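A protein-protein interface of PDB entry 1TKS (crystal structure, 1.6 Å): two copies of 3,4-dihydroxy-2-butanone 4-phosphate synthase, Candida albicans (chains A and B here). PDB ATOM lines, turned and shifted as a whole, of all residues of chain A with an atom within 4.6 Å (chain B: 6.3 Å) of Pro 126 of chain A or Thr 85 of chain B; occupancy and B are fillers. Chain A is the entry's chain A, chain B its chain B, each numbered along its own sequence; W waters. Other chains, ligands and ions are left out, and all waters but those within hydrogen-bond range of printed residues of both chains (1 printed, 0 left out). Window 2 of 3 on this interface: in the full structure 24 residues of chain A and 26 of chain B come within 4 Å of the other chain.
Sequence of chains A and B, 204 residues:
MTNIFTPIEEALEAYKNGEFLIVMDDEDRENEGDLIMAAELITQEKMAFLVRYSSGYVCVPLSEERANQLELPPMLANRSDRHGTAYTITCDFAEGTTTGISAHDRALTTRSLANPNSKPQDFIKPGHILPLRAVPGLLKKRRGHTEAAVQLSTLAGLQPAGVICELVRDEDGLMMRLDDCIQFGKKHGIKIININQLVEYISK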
ATOM      1  N   ILE A  89     -24.655 -18.340   3.370  1.00  0.00           N
ATOM      2  CA  ILE A  89     -23.943 -17.204   3.931  1.00  0.00           C
ATOM      3  C   ILE A  89     -24.316 -16.033   3.018  1.00  0.00           C
ATOM      4  O   ILE A  89     -24.491 -16.219   1.815  1.00  0.00           O
ATOM      5  CB  ILE A  89     -22.416 -17.432   3.902  1.00  0.00           C
ATOM      6  CG1 ILE A  89     -21.708 -16.258   4.573  1.00  0.00           C
ATOM      7  CG2 ILE A  89     -21.940 -17.590   2.462  1.00  0.00           C
ATOM      8  CD1 ILE A  89     -20.249 -16.521   4.878  1.00  0.00           C
ATOM      9  N   THR A  90     -24.455 -14.836   3.580  1.00  0.00           N
ATOM     10  CA  THR A  90     -24.823 -13.675   2.773  1.00  0.00           C
ATOM     11  C   THR A  90     -23.668 -13.209   1.896  1.00  0.00           C
ATOM     12  O   THR A  90     -22.518 -13.579   2.125  1.00  0.00           O
ATOM     13  CB  THR A  90     -25.305 -12.513   3.659  1.00  0.00           C
ATOM     14  OG1 THR A  90     -24.275 -12.158   4.590  1.00  0.00           O
ATOM     15  CG2 THR A  90     -26.564 -12.921   4.418  1.00  0.00           C
ATOM     16  N   CYS A  91     -23.964 -12.390   0.892  1.00  0.00           N
ATOM     17  CA  CYS A  91     -22.910 -11.937  -0.002  1.00  0.00           C
ATOM     18  C   CYS A  91     -23.204 -10.626  -0.721  1.00  0.00           C
ATOM     19  O   CYS A  91     -24.339 -10.157  -0.755  1.00  0.00           O
ATOM     20  CB  CYS A  91     -22.637 -13.025  -1.049  1.00  0.00           C
ATOM     21  SG  CYS A  91     -23.997 -13.279  -2.242  1.00  0.00           S
ATOM     22  N   ILE A 124     -18.190 -11.002  -2.065  1.00  0.00           N
ATOM     23  CA  ILE A 124     -17.655 -10.780  -0.736  1.00  0.00           C
ATOM     24  C   ILE A 124     -18.689 -11.357   0.215  1.00  0.00           C
ATOM     25  O   ILE A 124     -19.891 -11.177   0.017  1.00  0.00           O
ATOM     26  CB  ILE A 124     -17.466  -9.280  -0.450  1.00  0.00           C
ATOM     27  CG1 ILE A 124     -16.446  -8.702  -1.432  1.00  0.00           C
ATOM     28  CG2 ILE A 124     -17.007  -9.072   0.988  1.00  0.00           C
ATOM     29  CD1 ILE A 124     -16.231  -7.218  -1.305  1.00  0.00           C
ATOM     30  N   LYS A 125     -18.215 -12.069   1.230  1.00  0.00           N
ATOM     31  CA  LYS A 125     -19.090 -12.691   2.214  1.00  0.00           C
ATOM     32  C   LYS A 125     -18.531 -12.422   3.607  1.00  0.00           C
ATOM     33  O   LYS A 125     -17.322 -12.506   3.823  1.00  0.00           O
ATOM     34  CB  LYS A 125     -19.158 -14.202   1.961  1.00  0.00           C
ATOM     35  CG  LYS A 125     -19.705 -14.559   0.580  1.00  0.00           C
ATOM     36  CD  LYS A 125     -19.519 -16.028   0.240  1.00  0.00           C
ATOM     37  CE  LYS A 125     -18.045 -16.388   0.131  1.00  0.00           C
ATOM     38  NZ  LYS A 125     -17.838 -17.770  -0.388  1.00  0.00           N
ATOM     39  N   PRO A 126     -19.397 -12.033   4.558  1.00  0.00           N
ATOM     40  CA  PRO A 126     -20.844 -11.857   4.380  1.00  0.00           C
ATOM     41  C   PRO A 126     -21.178 -10.612   3.553  1.00  0.00           C
ATOM     42  O   PRO A 126     -20.294  -9.827   3.204  1.00  0.00           O
ATOM     43  CB  PRO A 126     -21.353 -11.748   5.817  1.00  0.00           C
ATOM     44  CG  PRO A 126     -20.209 -11.087   6.519  1.00  0.00           C
ATOM     45  CD  PRO A 126     -19.022 -11.845   5.972  1.00  0.00           C
ATOM     46  N   GLY A 127     -22.460 -10.449   3.246  1.00  0.00           N
ATOM     47  CA  GLY A 127     -22.893  -9.311   2.465  1.00  0.00           C
ATOM     48  C   GLY A 127     -24.282  -8.825   2.823  1.00  0.00           C
ATOM     49  O   GLY A 127     -24.745  -9.012   3.951  1.00  0.00           O
ATOM     50  N   MET B  75     -20.772 -14.891  11.343  1.00  0.00           N
ATOM     51  CA  MET B  75     -21.322 -15.665  10.245  1.00  0.00           C
ATOM     52  C   MET B  75     -20.209 -16.417   9.528  1.00  0.00           C
ATOM     53  O   MET B  75     -20.398 -17.550   9.082  1.00  0.00           O
ATOM     54  CB  MET B  75     -22.036 -14.735   9.272  1.00  0.00           C
ATOM     55  CG  MET B  75     -22.910 -15.443   8.275  1.00  0.00           C
ATOM     56  SD  MET B  75     -23.726 -14.229   7.249  1.00  0.00           S
ATOM     57  CE  MET B  75     -25.111 -13.757   8.295  1.00  0.00           C
ATOM     58  N   LEU B  76     -19.048 -15.775   9.425  1.00  0.00           N
ATOM     59  CA  LEU B  76     -17.891 -16.372   8.770  1.00  0.00           C
ATOM     60  C   LEU B  76     -16.809 -16.643   9.812  1.00  0.00           C
ATOM     61  O   LEU B  76     -16.258 -15.716  10.404  1.00  0.00           O
ATOM     62  CB  LEU B  76     -17.357 -15.429   7.686  1.00  0.00           C
ATOM     63  CG  LEU B  76     -16.331 -15.967   6.678  1.00  0.00           C
ATOM     64  CD1 LEU B  76     -14.968 -16.142   7.332  1.00  0.00           C
ATOM     65  CD2 LEU B  76     -16.837 -17.282   6.109  1.00  0.00           C
ATOM     66  N   GLY B  84     -21.661  -2.861   8.291  1.00  0.00           N
ATOM     67  CA  GLY B  84     -20.221  -2.981   8.419  1.00  0.00           C
ATOM     68  C   GLY B  84     -19.795  -4.387   8.787  1.00  0.00           C
ATOM     69  O   GLY B  84     -19.153  -4.598   9.816  1.00  0.00           O
ATOM     70  N   THR B  85     -20.155  -5.347   7.938  1.00  0.00           N
ATOM     71  CA  THR B  85     -19.829  -6.756   8.148  1.00  0.00           C
ATOM     72  C   THR B  85     -19.862  -7.138   9.630  1.00  0.00           C
ATOM     73  O   THR B  85     -20.698  -6.639  10.382  1.00  0.00           O
ATOM     74  CB  THR B  85     -18.447  -7.112   7.531  1.00  0.00           C
ATOM     75  OG1 THR B  85     -18.209  -8.520   7.657  1.00  0.00           O
ATOM     76  CG2 THR B  85     -17.332  -6.347   8.220  1.00  0.00           C
ATOM     77  N   ALA B  86     -18.962  -8.019  10.051  1.00  0.00           N
ATOM     78  CA  ALA B  86     -18.924  -8.457  11.443  1.00  0.00           C
ATOM     79  C   ALA B  86     -20.288  -9.010  11.863  1.00  0.00           C
ATOM     80  O   ALA B  86     -20.676  -8.936  13.033  1.00  0.00           O
ATOM     81  CB  ALA B  86     -18.526  -7.296  12.350  1.00  0.00           C
ATOM     82  N   TYR B  87     -21.016  -9.555  10.894  1.00  0.00           N
ATOM     83  CA  TYR B  87     -22.328 -10.138  11.151  1.00  0.00           C
ATOM     84  C   TYR B  87     -22.177 -11.466  11.874  1.00  0.00           C
ATOM     85  O   TYR B  87     -21.136 -12.115  11.781  1.00  0.00           O
ATOM     86  CB  TYR B  87     -23.066 -10.432   9.844  1.00  0.00           C
ATOM     87  CG  TYR B  87     -23.380  -9.239   8.982  1.00  0.00           C
ATOM     88  CD1 TYR B  87     -22.477  -8.794   8.017  1.00  0.00           C
ATOM     89  CD2 TYR B  87     -24.595  -8.571   9.110  1.00  0.00           C
ATOM     90  CE1 TYR B  87     -22.781  -7.715   7.194  1.00  0.00           C
ATOM     91  CE2 TYR B  87     -24.909  -7.492   8.298  1.00  0.00           C
ATOM     92  CZ  TYR B  87     -24.002  -7.070   7.342  1.00  0.00           C
ATOM     93  OH  TYR B  87     -24.313  -6.010   6.525  1.00  0.00           O
ATOM     94  N   THR B  88     -23.224 -11.871  12.584  1.00  0.00           N
ATOM     95  CA  THR B  88     -23.228 -13.160  13.266  1.00  0.00           C
ATOM     96  C   THR B  88     -24.294 -13.947  12.520  1.00  0.00           C
ATOM     97  O   THR B  88     -24.962 -13.406  11.633  1.00  0.00           O
ATOM     98  CB  THR B  88     -23.674 -13.063  14.747  1.00  0.00           C
ATOM     99  OG1 THR B  88     -25.094 -12.867  14.816  1.00  0.00           O
ATOM    100  CG2 THR B  88     -22.977 -11.915  15.439  1.00  0.00           C
ATOM    101  N   LEU B 132     -25.248  -7.920  15.216  1.00  0.00           N
ATOM    102  CA  LEU B 132     -23.933  -7.396  14.849  1.00  0.00           C
ATOM    103  C   LEU B 132     -23.067  -7.340  16.098  1.00  0.00           C
ATOM    104  O   LEU B 132     -23.552  -6.986  17.169  1.00  0.00           O
ATOM    105  CB  LEU B 132     -24.053  -5.991  14.261  1.00  0.00           C
ATOM    106  CG  LEU B 132     -24.968  -5.827  13.050  1.00  0.00           C
ATOM    107  CD1 LEU B 132     -24.807  -4.425  12.483  1.00  0.00           C
ATOM    108  CD2 LEU B 132     -24.628  -6.868  12.000  1.00  0.00           C
ATOM    109  N   ARG B 133     -21.790  -7.687  15.961  1.00  0.00           N
ATOM    110  CA  ARG B 133     -20.877  -7.682  17.100  1.00  0.00           C
ATOM    111  C   ARG B 133     -20.064  -6.399  17.231  1.00  0.00           C
ATOM    112  O   ARG B 133     -19.187  -6.123  16.411  1.00  0.00           O
ATOM    113  CB  ARG B 133     -19.924  -8.877  17.011  1.00  0.00           C
ATOM    114  CG  ARG B 133     -20.618 -10.225  17.110  1.00  0.00           C
ATOM    115  CD  ARG B 133     -19.614 -11.368  17.101  1.00  0.00           C
ATOM    116  NE  ARG B 133     -18.802 -11.344  18.315  1.00  0.00           N
ATOM    117  CZ  ARG B 133     -17.930 -12.285  18.660  1.00  0.00           C
ATOM    118  NH1 ARG B 133     -17.742 -13.342  17.882  1.00  0.00           N
ATOM    119  NH2 ARG B 133     -17.247 -12.169  19.790  1.00  0.00           N
ATOM    120  N   ARG B 142     -13.615   1.686  17.454  1.00  0.00           N
ATOM    121  CA  ARG B 142     -14.088   1.652  16.069  1.00  0.00           C
ATOM    122  C   ARG B 142     -15.308   2.558  15.941  1.00  0.00           C
ATOM    123  O   ARG B 142     -16.294   2.378  16.655  1.00  0.00           O
ATOM    124  CB  ARG B 142     -14.464   0.217  15.684  1.00  0.00           C
ATOM    125  CG  ARG B 142     -14.981   0.058  14.261  1.00  0.00           C
ATOM    126  CD  ARG B 142     -15.228  -1.414  13.931  1.00  0.00           C
ATOM    127  NE  ARG B 142     -15.635  -1.614  12.538  1.00  0.00           N
ATOM    128  CZ  ARG B 142     -16.876  -1.471  12.080  1.00  0.00           C
ATOM    129  NH1 ARG B 142     -17.132  -1.673  10.794  1.00  0.00           N
ATOM    130  NH2 ARG B 142     -17.865  -1.147  12.901  1.00  0.00           N
ATOM    131  N   THR B 146     -22.397   0.240  14.437  1.00  0.00           N
ATOM    132  CA  THR B 146     -22.647  -0.881  15.334  1.00  0.00           C
ATOM    133  C   THR B 146     -22.187  -0.460  16.721  1.00  0.00           C
ATOM    134  O   THR B 146     -22.930  -0.582  17.699  1.00  0.00           O
ATOM    135  CB  THR B 146     -21.864  -2.134  14.901  1.00  0.00           C
ATOM    136  OG1 THR B 146     -22.347  -2.575  13.630  1.00  0.00           O
ATOM    137  CG2 THR B 146     -22.039  -3.257  15.916  1.00  0.00           C
HETATM  138  O   HOH W   1     -18.061  -8.520   4.756  1.00  0.00           O
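The side-chain sulfur of Met 75 of chain B sits at hydrogen-bond distance from the side-chain hydroxyl of Thr 90 of chain A.
The backbone NH (N) of Gly 127 of chain A is in hydrogen-bond range of the side-chain hydroxyl (OG1) of Thr 90 of chain A (2.8 Å). The backbone NH of Met 75 of chain B is in hydrogen-bond range of the backbone carbonyl oxygen of Tyr 87 of chain B (2.8 Å).
Water W1 bridges the side-chain hydroxyl of Thr 85 of chain B and the backbone carbonyl oxygen of Pro 126 of chain A.
Among the printed residues, merely in contact across the chains: Ile 89 of chain A with Met 75 of chain B, Ile 89 of chain A with Leu 76 of chain B, Pro 126 of chain A with Met 75 of chain B, Pro 126 of chain A with Thr 85 of chain B, Pro 126 of chain A with Tyr 87 of chain B and Gly 127 of chain A with Tyr 87 of chain B.
Hydrophobic or aromatic side chains of chain B within 4 Å of the printed part of chain A: Met 75, Leu 76 and Tyr 87. Printed residues of chain A that touch a printed residue of chain B: Ile 89, Thr 90, Pro 126 and Gly 127. Hydrophobic or aromatic side chains of chain A that line the printed part of chain B: Ile 89 and Pro 126. Among the printed residues, 7 pairs touch across the chains.
No position is printed for both chains. Of the 7 pairs that touch across the chains among the printed residues, none has its exchanged pair printed and touching as well.
Of the printed residues of chain B, Pro 126 of chain A touches Met 75 (3.7 Å), Thr 85 (3.4 Å) and Tyr 87 (3.6 Å). Of chain A, only Pro 126 (3.4 Å) comes within 4 Å of Thr 85 of chain B. Of the printed residues of chain A, Leu 76 of chain B touches Ile 89. Of the printed residues of chain B, Gly 127 of chain A touches Tyr 87 (3.98 Å). Gly 84 of chain B touches none of the printed residues of chain A. Leu 132 of chain B touches none of the printed residues of chain A. The nearest residue of chain B that does not touch Pro 126 of chain A is Leu 76 of chain B (4.3 Å). The nearest printed residue of chain A that does not touch Thr 85 of chain B is Lys 125 of chain A (5.6 Å).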
